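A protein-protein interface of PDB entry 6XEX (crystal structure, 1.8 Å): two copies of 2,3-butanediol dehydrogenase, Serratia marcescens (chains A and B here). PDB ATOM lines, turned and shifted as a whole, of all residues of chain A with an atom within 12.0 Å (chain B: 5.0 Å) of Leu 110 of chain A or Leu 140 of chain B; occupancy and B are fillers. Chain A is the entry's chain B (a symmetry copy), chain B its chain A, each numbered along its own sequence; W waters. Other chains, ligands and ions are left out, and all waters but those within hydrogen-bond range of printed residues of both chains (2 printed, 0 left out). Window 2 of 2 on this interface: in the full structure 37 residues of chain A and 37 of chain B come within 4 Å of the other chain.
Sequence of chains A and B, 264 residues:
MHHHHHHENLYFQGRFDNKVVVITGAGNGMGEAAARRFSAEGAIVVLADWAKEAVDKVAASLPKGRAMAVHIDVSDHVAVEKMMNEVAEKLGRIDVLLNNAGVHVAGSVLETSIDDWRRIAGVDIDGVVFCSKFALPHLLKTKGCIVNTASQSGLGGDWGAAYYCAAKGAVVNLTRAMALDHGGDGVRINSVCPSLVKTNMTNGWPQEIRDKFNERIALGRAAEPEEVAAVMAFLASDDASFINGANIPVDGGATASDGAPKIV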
ATOM      1  N   VAL A 105      25.935  32.963  -8.894  1.00  0.00           N
ATOM      2  CA  VAL A 105      25.027  31.885  -9.357  1.00  0.00           C
ATOM      3  C   VAL A 105      23.600  32.387  -9.139  1.00  0.00           C
ATOM      4  O   VAL A 105      23.316  32.955  -8.068  1.00  0.00           O
ATOM      5  CB  VAL A 105      25.302  30.574  -8.609  1.00  0.00           C
ATOM      6  CG1 VAL A 105      24.338  29.481  -9.035  1.00  0.00           C
ATOM      7  CG2 VAL A 105      26.727  30.081  -8.799  1.00  0.00           C
ATOM      8  N   ALA A 106      22.736  32.247 -10.141  1.00  0.00           N
ATOM      9  CA  ALA A 106      21.324  32.664 -10.065  1.00  0.00           C
ATOM     10  C   ALA A 106      20.500  31.575  -9.360  1.00  0.00           C
ATOM     11  O   ALA A 106      20.774  30.375  -9.535  1.00  0.00           O
ATOM     12  CB  ALA A 106      20.789  33.017 -11.445  1.00  0.00           C
ATOM     13  N   GLY A 107      19.527  32.007  -8.558  1.00  0.00           N
ATOM     14  CA  GLY A 107      18.459  31.167  -8.003  1.00  0.00           C
ATOM     15  C   GLY A 107      18.131  31.511  -6.560  1.00  0.00           C
ATOM     16  O   GLY A 107      18.987  32.101  -5.868  1.00  0.00           O
ATOM     17  N   SER A 108      16.923  31.150  -6.132  1.00  0.00           N
ATOM     18  CA  SER A 108      16.576  31.051  -4.694  1.00  0.00           C
ATOM     19  C   SER A 108      17.377  29.903  -4.100  1.00  0.00           C
ATOM     20  O   SER A 108      18.007  29.126  -4.885  1.00  0.00           O
ATOM     21  CB  SER A 108      15.102  30.857  -4.509  1.00  0.00           C
ATOM     22  OG  SER A 108      14.727  29.558  -4.946  1.00  0.00           O
ATOM     23  N   VAL A 109      17.300  29.725  -2.787  1.00  0.00           N
ATOM     24  CA  VAL A 109      17.947  28.579  -2.088  1.00  0.00           C
ATOM     25  C   VAL A 109      17.319  27.257  -2.567  1.00  0.00           C
ATOM     26  O   VAL A 109      17.937  26.210  -2.332  1.00  0.00           O
ATOM     27  CB  VAL A 109      17.827  28.688  -0.559  1.00  0.00           C
ATOM     28  CG1 VAL A 109      18.423  30.009  -0.056  1.00  0.00           C
ATOM     29  CG2 VAL A 109      16.386  28.513  -0.102  1.00  0.00           C
ATOM     30  N   LEU A 110      16.110  27.292  -3.113  1.00  0.00           N
ATOM     31  CA  LEU A 110      15.444  26.049  -3.602  1.00  0.00           C
ATOM     32  C   LEU A 110      15.923  25.728  -5.026  1.00  0.00           C
ATOM     33  O   LEU A 110      15.620  24.630  -5.512  1.00  0.00           O
ATOM     34  CB  LEU A 110      13.929  26.237  -3.575  1.00  0.00           C
ATOM     35  CG  LEU A 110      13.277  26.431  -2.205  1.00  0.00           C
ATOM     36  CD1 LEU A 110      11.770  26.520  -2.367  1.00  0.00           C
ATOM     37  CD2 LEU A 110      13.655  25.344  -1.205  1.00  0.00           C
ATOM     38  N   GLU A 111      16.611  26.646  -5.690  1.00  0.00           N
ATOM     39  CA  GLU A 111      17.027  26.504  -7.107  1.00  0.00           C
ATOM     40  C   GLU A 111      18.538  26.300  -7.147  1.00  0.00           C
ATOM     41  O   GLU A 111      19.067  26.055  -8.224  1.00  0.00           O
ATOM     42  CB  GLU A 111      16.572  27.730  -7.896  1.00  0.00           C
ATOM     43  CG  GLU A 111      15.081  27.822  -8.120  1.00  0.00           C
ATOM     44  CD  GLU A 111      14.645  29.159  -8.670  1.00  0.00           C
ATOM     45  OE1 GLU A 111      15.276  30.170  -8.309  1.00  0.00           O
ATOM     46  OE2 GLU A 111      13.690  29.202  -9.490  1.00  0.00           O
ATOM     47  N   THR A 112      19.229  26.454  -6.016  1.00  0.00           N
ATOM     48  CA  THR A 112      20.709  26.437  -5.959  1.00  0.00           C
ATOM     49  C   THR A 112      21.110  25.406  -4.928  1.00  0.00           C
ATOM     50  O   THR A 112      20.395  25.261  -3.921  1.00  0.00           O
ATOM     51  CB  THR A 112      21.311  27.824  -5.700  1.00  0.00           C
ATOM     52  OG1 THR A 112      20.601  28.415  -4.612  1.00  0.00           O
ATOM     53  CG2 THR A 112      21.218  28.719  -6.908  1.00  0.00           C
ATOM     54  N   SER A 113      22.217  24.719  -5.198  1.00  0.00           N
ATOM     55  CA  SER A 113      22.723  23.525  -4.485  1.00  0.00           C
ATOM     56  C   SER A 113      23.676  23.923  -3.361  1.00  0.00           C
ATOM     57  O   SER A 113      24.138  25.065  -3.381  1.00  0.00           O
ATOM     58  CB  SER A 113      23.438  22.638  -5.464  1.00  0.00           C
ATOM     59  OG  SER A 113      24.432  23.374  -6.173  1.00  0.00           O
ATOM     60  N   ILE A 114      24.046  22.965  -2.511  1.00  0.00           N
ATOM     61  CA  ILE A 114      25.145  23.121  -1.520  1.00  0.00           C
ATOM     62  C   ILE A 114      26.418  23.509  -2.280  1.00  0.00           C
ATOM     63  O   ILE A 114      27.186  24.350  -1.767  1.00  0.00           O
ATOM     64  CB  ILE A 114      25.385  21.858  -0.668  1.00  0.00           C
ATOM     65  CG1 ILE A 114      24.142  21.340   0.070  1.00  0.00           C
ATOM     66  CG2 ILE A 114      26.538  22.079   0.302  1.00  0.00           C
ATOM     67  CD1 ILE A 114      23.311  22.398   0.725  1.00  0.00           C
ATOM     68  N   ASP A 115      26.646  22.917  -3.457  1.00  0.00           N
ATOM     69  CA  ASP A 115      27.880  23.195  -4.235  1.00  0.00           C
ATOM     70  C   ASP A 115      27.851  24.668  -4.620  1.00  0.00           C
ATOM     71  O   ASP A 115      28.907  25.306  -4.553  1.00  0.00           O
ATOM     72  CB  ASP A 115      28.011  22.284  -5.465  1.00  0.00           C
ATOM     73  CG  ASP A 115      29.302  22.477  -6.240  1.00  0.00           C
ATOM     74  OD1 ASP A 115      30.372  22.198  -5.656  1.00  0.00           O
ATOM     75  OD2 ASP A 115      29.206  22.885  -7.448  1.00  0.00           O
ATOM     76  N   ASP A 116      26.706  25.138  -5.098  1.00  0.00           N
ATOM     77  CA  ASP A 116      26.550  26.543  -5.524  1.00  0.00           C
ATOM     78  C   ASP A 116      26.867  27.420  -4.298  1.00  0.00           C
ATOM     79  O   ASP A 116      27.605  28.403  -4.452  1.00  0.00           O
ATOM     80  CB  ASP A 116      25.164  26.836  -6.088  1.00  0.00           C
ATOM     81  CG  ASP A 116      24.820  26.183  -7.413  1.00  0.00           C
ATOM     82  OD1 ASP A 116      25.727  26.006  -8.230  1.00  0.00           O
ATOM     83  OD2 ASP A 116      23.625  25.892  -7.590  1.00  0.00           O
ATOM     84  N   TRP A 117      26.392  27.045  -3.112  1.00  0.00           N
ATOM     85  CA  TRP A 117      26.693  27.814  -1.871  1.00  0.00           C
ATOM     86  C   TRP A 117      28.209  27.849  -1.615  1.00  0.00           C
ATOM     87  O   TRP A 117      28.753  28.935  -1.384  1.00  0.00           O
ATOM     88  CB  TRP A 117      25.927  27.244  -0.671  1.00  0.00           C
ATOM     89  CG  TRP A 117      26.406  27.800   0.633  1.00  0.00           C
ATOM     90  CD1 TRP A 117      27.011  27.154   1.659  1.00  0.00           C
ATOM     91  CD2 TRP A 117      26.371  29.196   1.007  1.00  0.00           C
ATOM     92  NE1 TRP A 117      27.330  28.035   2.653  1.00  0.00           N
ATOM     93  CE2 TRP A 117      26.954  29.292   2.276  1.00  0.00           C
ATOM     94  CE3 TRP A 117      25.902  30.350   0.389  1.00  0.00           C
ATOM     95  CZ2 TRP A 117      27.077  30.511   2.946  1.00  0.00           C
ATOM     96  CZ3 TRP A 117      26.009  31.558   1.050  1.00  0.00           C
ATOM     97  CH2 TRP A 117      26.558  31.613   2.324  1.00  0.00           C
ATOM     98  N   ILE A 120      30.054  30.164  -4.153  1.00  0.00           N
ATOM     99  CA  ILE A 120      29.825  31.609  -3.898  1.00  0.00           C
ATOM    100  C   ILE A 120      30.561  31.987  -2.603  1.00  0.00           C
ATOM    101  O   ILE A 120      31.290  33.012  -2.611  1.00  0.00           O
ATOM    102  CB  ILE A 120      28.314  31.886  -3.894  1.00  0.00           C
ATOM    103  CG1 ILE A 120      27.795  32.148  -5.303  1.00  0.00           C
ATOM    104  CG2 ILE A 120      27.969  33.074  -2.977  1.00  0.00           C
ATOM    105  CD1 ILE A 120      26.319  31.949  -5.384  1.00  0.00           C
ATOM    106  N   ASP A 158      18.036  40.653  -3.531  1.00  0.00           N
ATOM    107  CA  ASP A 158      17.559  40.504  -4.926  1.00  0.00           C
ATOM    108  C   ASP A 158      16.488  39.413  -4.899  1.00  0.00           C
ATOM    109  O   ASP A 158      16.602  38.539  -4.031  1.00  0.00           O
ATOM    110  CB  ASP A 158      18.677  39.983  -5.822  1.00  0.00           C
ATOM    111  CG  ASP A 158      19.817  40.950  -6.038  1.00  0.00           C
ATOM    112  OD1 ASP A 158      19.519  42.132  -6.211  1.00  0.00           O
ATOM    113  OD2 ASP A 158      20.975  40.473  -6.096  1.00  0.00           O
ATOM    114  N   TRP A 159      15.612  39.393  -5.901  1.00  0.00           N
ATOM    115  CA  TRP A 159      14.865  38.166  -6.275  1.00  0.00           C
ATOM    116  C   TRP A 159      15.824  37.245  -7.035  1.00  0.00           C
ATOM    117  O   TRP A 159      16.491  37.731  -7.922  1.00  0.00           O
ATOM    118  CB  TRP A 159      13.650  38.476  -7.131  1.00  0.00           C
ATOM    119  CG  TRP A 159      12.495  39.121  -6.433  1.00  0.00           C
ATOM    120  CD1 TRP A 159      11.398  38.492  -5.919  1.00  0.00           C
ATOM    121  CD2 TRP A 159      12.262  40.532  -6.261  1.00  0.00           C
ATOM    122  NE1 TRP A 159      10.512  39.409  -5.432  1.00  0.00           N
ATOM    123  CE2 TRP A 159      11.017  40.666  -5.610  1.00  0.00           C
ATOM    124  CE3 TRP A 159      12.996  41.692  -6.542  1.00  0.00           C
ATOM    125  CZ2 TRP A 159      10.478  41.903  -5.288  1.00  0.00           C
ATOM    126  CZ3 TRP A 159      12.466  42.917  -6.199  1.00  0.00           C
ATOM    127  CH2 TRP A 159      11.241  43.014  -5.549  1.00  0.00           C
ATOM    128  N   GLY A 160      15.974  36.003  -6.605  1.00  0.00           N
ATOM    129  CA  GLY A 160      16.634  34.943  -7.392  1.00  0.00           C
ATOM    130  C   GLY A 160      18.142  35.025  -7.342  1.00  0.00           C
ATOM    131  O   GLY A 160      18.783  34.716  -8.366  1.00  0.00           O
ATOM    132  N   ALA A 161      18.725  35.345  -6.184  1.00  0.00           N
ATOM    133  CA  ALA A 161      20.195  35.282  -5.994  1.00  0.00           C
ATOM    134  C   ALA A 161      20.510  35.186  -4.506  1.00  0.00           C
ATOM    135  O   ALA A 161      21.258  36.065  -4.012  1.00  0.00           O
ATOM    136  CB  ALA A 161      20.840  36.499  -6.633  1.00  0.00           C
ATOM    137  N   ALA A 162      19.945  34.189  -3.810  1.00  0.00           N
ATOM    138  CA  ALA A 162      19.872  34.224  -2.325  1.00  0.00           C
ATOM    139  C   ALA A 162      21.276  34.055  -1.732  1.00  0.00           C
ATOM    140  O   ALA A 162      21.703  34.825  -0.804  1.00  0.00           O
ATOM    141  CB  ALA A 162      18.908  33.162  -1.848  1.00  0.00           C
ATOM    142  N   TYR A 163      22.003  33.045  -2.196  1.00  0.00           N
ATOM    143  CA  TYR A 163      23.392  32.807  -1.736  1.00  0.00           C
ATOM    144  C   TYR A 163      24.276  34.027  -2.017  1.00  0.00           C
ATOM    145  O   TYR A 163      25.107  34.379  -1.151  1.00  0.00           O
ATOM    146  CB  TYR A 163      24.055  31.620  -2.422  1.00  0.00           C
ATOM    147  CG  TYR A 163      23.385  30.304  -2.130  1.00  0.00           C
ATOM    148  CD1 TYR A 163      22.523  30.129  -1.054  1.00  0.00           C
ATOM    149  CD2 TYR A 163      23.585  29.228  -2.978  1.00  0.00           C
ATOM    150  CE1 TYR A 163      21.911  28.919  -0.816  1.00  0.00           C
ATOM    151  CE2 TYR A 163      22.950  28.024  -2.766  1.00  0.00           C
ATOM    152  CZ  TYR A 163      22.107  27.869  -1.694  1.00  0.00           C
ATOM    153  OH  TYR A 163      21.484  26.684  -1.481  1.00  0.00           O
ATOM    154  N   TYR A 164      24.124  34.623  -3.198  1.00  0.00           N
ATOM    155  CA  TYR A 164      24.962  35.770  -3.639  1.00  0.00           C
ATOM    156  C   TYR A 164      24.733  36.944  -2.667  1.00  0.00           C
ATOM    157  O   TYR A 164      25.655  37.636  -2.284  1.00  0.00           O
ATOM    158  CB  TYR A 164      24.604  36.196  -5.060  1.00  0.00           C
ATOM    159  CG  TYR A 164      25.504  37.264  -5.632  1.00  0.00           C
ATOM    160  CD1 TYR A 164      26.825  36.990  -5.951  1.00  0.00           C
ATOM    161  CD2 TYR A 164      25.027  38.533  -5.899  1.00  0.00           C
ATOM    162  CE1 TYR A 164      27.648  37.942  -6.529  1.00  0.00           C
ATOM    163  CE2 TYR A 164      25.850  39.518  -6.443  1.00  0.00           C
ATOM    164  CZ  TYR A 164      27.158  39.212  -6.783  1.00  0.00           C
ATOM    165  OH  TYR A 164      27.979  40.166  -7.323  1.00  0.00           O
ATOM    166  N   LYS B 133      16.887  26.170   4.003  1.00  0.00           N
ATOM    167  CA  LYS B 133      16.766  25.512   2.678  1.00  0.00           C
ATOM    168  C   LYS B 133      15.915  24.239   2.896  1.00  0.00           C
ATOM    169  O   LYS B 133      15.008  23.991   2.107  1.00  0.00           O
ATOM    170  CB  LYS B 133      18.150  25.242   2.068  1.00  0.00           C
ATOM    171  CG  LYS B 133      18.170  24.350   0.806  1.00  0.00           C
ATOM    172  CD  LYS B 133      19.584  24.163   0.197  1.00  0.00           C
ATOM    173  CE  LYS B 133      19.681  23.247  -1.031  1.00  0.00           C
ATOM    174  NZ  LYS B 133      18.802  23.709  -2.119  1.00  0.00           N
ATOM    175  N   LEU B 136      12.094  24.827   4.087  1.00  0.00           N
ATOM    176  CA  LEU B 136      11.235  25.640   3.203  1.00  0.00           C
ATOM    177  C   LEU B 136      10.140  24.809   2.526  1.00  0.00           C
ATOM    178  O   LEU B 136       9.006  25.252   2.495  1.00  0.00           O
ATOM    179  CB  LEU B 136      12.081  26.372   2.162  1.00  0.00           C
ATOM    180  CG  LEU B 136      12.154  27.870   2.387  1.00  0.00           C
ATOM    181  CD1 LEU B 136      13.321  28.438   1.591  1.00  0.00           C
ATOM    182  CD2 LEU B 136      10.839  28.558   2.036  1.00  0.00           C
ATOM    183  N   PRO B 137      10.420  23.630   1.934  1.00  0.00           N
ATOM    184  CA  PRO B 137       9.366  22.875   1.238  1.00  0.00           C
ATOM    185  C   PRO B 137       8.163  22.634   2.169  1.00  0.00           C
ATOM    186  O   PRO B 137       7.002  22.793   1.758  1.00  0.00           O
ATOM    187  CB  PRO B 137      10.074  21.584   0.793  1.00  0.00           C
ATOM    188  CG  PRO B 137      11.540  21.953   0.754  1.00  0.00           C
ATOM    189  CD  PRO B 137      11.722  22.943   1.897  1.00  0.00           C
ATOM    190  N   HIS B 138       8.453  22.378   3.432  1.00  0.00           N
ATOM    191  CA  HIS B 138       7.453  22.107   4.501  1.00  0.00           C
ATOM    192  C   HIS B 138       6.709  23.389   4.917  1.00  0.00           C
ATOM    193  O   HIS B 138       5.475  23.379   5.022  1.00  0.00           O
ATOM    194  CB  HIS B 138       8.154  21.410   5.674  1.00  0.00           C
ATOM    195  CG  HIS B 138       8.883  20.167   5.312  1.00  0.00           C
ATOM    196  ND1 HIS B 138       8.249  19.096   4.708  1.00  0.00           N
ATOM    197  CD2 HIS B 138      10.183  19.814   5.481  1.00  0.00           C
ATOM    198  CE1 HIS B 138       9.134  18.136   4.525  1.00  0.00           C
ATOM    199  NE2 HIS B 138      10.330  18.537   5.002  1.00  0.00           N
ATOM    200  N   LEU B 139       7.427  24.498   5.132  1.00  0.00           N
ATOM    201  CA  LEU B 139       6.807  25.824   5.433  1.00  0.00           C
ATOM    202  C   LEU B 139       5.935  26.263   4.246  1.00  0.00           C
ATOM    203  O   LEU B 139       4.907  26.941   4.448  1.00  0.00           O
ATOM    204  CB  LEU B 139       7.919  26.860   5.710  1.00  0.00           C
ATOM    205  CG  LEU B 139       8.871  26.585   6.872  1.00  0.00           C
ATOM    206  CD1 LEU B 139      10.080  27.533   6.818  1.00  0.00           C
ATOM    207  CD2 LEU B 139       8.137  26.791   8.181  1.00  0.00           C
ATOM    208  N   LEU B 140       6.288  25.927   3.005  1.00  0.00           N
ATOM    209  CA  LEU B 140       5.447  26.387   1.865  1.00  0.00           C
ATOM    210  C   LEU B 140       4.062  25.734   1.976  1.00  0.00           C
ATOM    211  O   LEU B 140       3.053  26.391   1.609  1.00  0.00           O
ATOM    212  CB  LEU B 140       6.145  26.037   0.549  1.00  0.00           C
ATOM    213  CG  LEU B 140       7.231  27.027   0.132  1.00  0.00           C
ATOM    214  CD1 LEU B 140       8.154  26.412  -0.915  1.00  0.00           C
ATOM    215  CD2 LEU B 140       6.599  28.301  -0.370  1.00  0.00           C
ATOM    216  N   LYS B 141       4.030  24.510   2.497  1.00  0.00           N
ATOM    217  CA  LYS B 141       2.768  23.715   2.630  1.00  0.00           C
ATOM    218  C   LYS B 141       1.872  24.338   3.697  1.00  0.00           C
ATOM    219  O   LYS B 141       0.678  24.365   3.492  1.00  0.00           O
ATOM    220  CB  LYS B 141       3.093  22.262   2.965  1.00  0.00           C
ATOM    221  CG  LYS B 141       3.617  21.470   1.779  1.00  0.00           C
ATOM    222  CD  LYS B 141       4.026  20.059   2.135  1.00  0.00           C
ATOM    223  CE  LYS B 141       5.139  19.557   1.238  1.00  0.00           C
ATOM    224  NZ  LYS B 141       5.786  18.342   1.788  1.00  0.00           N
ATOM    225  N   THR B 142       2.452  24.944   4.733  1.00  0.00           N
ATOM    226  CA  THR B 142       1.682  25.542   5.849  1.00  0.00           C
ATOM    227  C   THR B 142       1.576  27.066   5.727  1.00  0.00           C
ATOM    228  O   THR B 142       0.900  27.655   6.571  1.00  0.00           O
ATOM    229  CB  THR B 142       2.319  25.141   7.180  1.00  0.00           C
ATOM    230  OG1 THR B 142       3.657  25.627   7.211  1.00  0.00           O
ATOM    231  CG2 THR B 142       2.327  23.649   7.391  1.00  0.00           C
ATOM    232  N   LYS B 143       2.162  27.696   4.704  1.00  0.00           N
ATOM    233  CA  LYS B 143       2.331  29.174   4.685  1.00  0.00           C
ATOM    234  C   LYS B 143       2.901  29.626   6.043  1.00  0.00           C
ATOM    235  O   LYS B 143       2.466  30.668   6.594  1.00  0.00           O
ATOM    236  CB  LYS B 143       1.013  29.809   4.248  1.00  0.00           C
ATOM    237  CG  LYS B 143       0.636  29.341   2.849  1.00  0.00           C
ATOM    238  CD  LYS B 143      -0.389  30.144   2.133  1.00  0.00           C
ATOM    239  CE  LYS B 143      -0.474  29.740   0.672  1.00  0.00           C
ATOM    240  NZ  LYS B 143      -0.934  30.877  -0.163  1.00  0.00           N
ATOM    241  N   HIS B 182      10.386  34.088  -1.417  1.00  0.00           N
ATOM    242  CA  HIS B 182       9.353  33.145  -0.917  1.00  0.00           C
ATOM    243  C   HIS B 182       8.125  33.841  -0.354  1.00  0.00           C
ATOM    244  O   HIS B 182       7.136  33.145  -0.085  1.00  0.00           O
ATOM    245  CB  HIS B 182       9.975  32.176   0.077  1.00  0.00           C
ATOM    246  CG  HIS B 182      11.180  31.524  -0.488  1.00  0.00           C
ATOM    247  ND1 HIS B 182      11.114  30.676  -1.585  1.00  0.00           N
ATOM    248  CD2 HIS B 182      12.486  31.672  -0.179  1.00  0.00           C
ATOM    249  CE1 HIS B 182      12.341  30.311  -1.894  1.00  0.00           C
ATOM    250  NE2 HIS B 182      13.205  30.885  -1.040  1.00  0.00           N
ATOM    251  N   ASP B 185       4.921  33.284  -2.133  1.00  0.00           N
ATOM    252  CA  ASP B 185       4.427  31.893  -2.013  1.00  0.00           C
ATOM    253  C   ASP B 185       3.913  31.669  -0.579  1.00  0.00           C
ATOM    254  O   ASP B 185       3.692  30.506  -0.228  1.00  0.00           O
ATOM    255  CB  ASP B 185       5.542  30.931  -2.422  1.00  0.00           C
ATOM    256  CG  ASP B 185       5.975  31.145  -3.872  1.00  0.00           C
ATOM    257  OD1 ASP B 185       5.064  31.332  -4.698  1.00  0.00           O
ATOM    258  OD2 ASP B 185       7.213  31.184  -4.153  1.00  0.00           O
ATOM    259  N   VAL B 187       5.384  32.510   2.455  1.00  0.00           N
ATOM    260  CA  VAL B 187       6.348  32.247   3.549  1.00  0.00           C
ATOM    261  C   VAL B 187       7.106  33.537   3.881  1.00  0.00           C
ATOM    262  O   VAL B 187       8.051  33.907   3.113  1.00  0.00           O
ATOM    263  CB  VAL B 187       7.296  31.093   3.223  1.00  0.00           C
ATOM    264  CG1 VAL B 187       8.416  30.970   4.239  1.00  0.00           C
ATOM    265  CG2 VAL B 187       6.525  29.787   3.104  1.00  0.00           C
HETATM  266  O   HOH W   1      15.897  31.803  -1.434  1.00  0.00           O
HETATM  267  O   HOH W   2      19.662  21.911  -4.187  1.00  0.00           O
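The backbone NH (N) of Val 187 of chain B sits at hydrogen-bond distance from the backbone carbonyl oxygen (O) of His 182 of chain B (3.2 Å). The side-chain hydroxyl of Ser 108 of chain A lies close to the backbone NH of Leu 110 of chain A (3.2 Å). OE1 of Glu 111 of chain A sits at hydrogen-bond distance from N of Ser 108 of chain A, at 2.9 Å. The side-chain hydroxyl (OG1) of Thr 112 of chain A lies within hydrogen-bond range of the backbone carbonyl oxygen (O) of Ser 108 of chain A, at 2.7 Å. The side-chain hydroxyl (OH) of Tyr 163 of chain A lies within hydrogen-bond range of the backbone carbonyl oxygen (O) of Thr 112 of chain A, 3.0 Å away.
No position is printed for both chains. Of the 9 pairs that touch across the chains among the printed residues, none has its exchanged pair printed and touching as well.
Of the printed residues of chain B, Ser 108 of chain A touches His 182 (3.8 Å). Of chain B, only Lys 133, Leu 136, Leu 140 and His 182 come within 4 Å of Leu 110 of chain A. Glu 111 of chain A touches none of the printed residues of chain B. Printed residues of chain B within 4 Å of Thr 112 of chain A: Lys 133. Trp 117 of chain A touches none of the printed residues of chain B. Of chain A, only Val 109 (2.7 Å), Leu 110 (3.8 Å), Thr 112 (2.9 Å) and Tyr 163 (3.6 Å) come within 4 Å of Lys 133 of chain B. Leu 136 of chain B touches two residues of chain A. No residue of chain A comes within 4 Å of Pro 137 of chain B. No residue of chain A comes within 4 Å of Leu 139 of chain B. Leu 140 of chain B touches just one residue of chain A: Leu 110 (3.9 Å). No residue of chain A comes within 4 Å of Lys 141 of chain B. Thr 142 of chain B touches none of the printed residues of chain A. No residue of chain A comes within 4 Å of Lys 143 of chain B. His 182 of chain B touches just these residues of chain A: Ser 108 (3.8 Å) and Leu 110 (3.9 Å). No residue of chain A comes within 4 Å of Asp 185 of chain B. No residue of chain A comes within 4 Å of Val 187 of chain B. The nearest residue of chain B that does not touch Leu 110 of chain A is Pro 137 of chain B (4.4 Å). The nearest residue of chain A that does not touch Leu 140 of chain B is Ser 108 of chain A (8.3 Å). The nearest printed residue of chain B that does not touch Tyr 163 of chain A is Leu 136 of chain B (8.9 Å).
The side-chain amino group (NZ) of Lys 133 of chain B sits at hydrogen-bond distance from the backbone carbonyl oxygen (O) of Val 109 of chain A. The side-chain amino group of Lys 133 of chain B is in hydrogen-bond range of the backbone carbonyl oxygen of Thr 112 of chain A, 2.9 Å away.
Among the printed residues, merely in contact across the chains: Val 109 of chain A with Leu 136 of chain B (3.5 Å), Tyr 163 of chain A with Lys 133 of chain B (3.6 Å), Leu 110 of chain A with Lys 133 of chain B (3.8 Å), Ser 108 of chain A with His 182 of chain B (3.8 Å), Leu 110 of chain A with Leu 136 of chain B (3.9 Å), Leu 110 of chain A with His 182 of chain B (3.9 Å) and Leu 110 of chain A with Leu 140 of chain B (3.9 Å).
Hydrophobic or aromatic side chains of chain A within 4 Å of the printed part of chain B: Val 109, Leu 110 and Tyr 163. Among the printed residues, 9 pairs touch across the chains. Among the printed residues, no Asp or Glu carboxylate lies within 4 Å of a Lys or Arg side-chain nitrogen of the other chain.
Water W1 bridges the backbone NH (N) of Val 109 of chain A (2.8 Å) and a ring nitrogen (NE2) of His 182 of chain B (2.9 Å). Water W2 lies within hydrogen-bond range of NZ of Lys 133 of chain B and O of Thr 112 of chain A.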
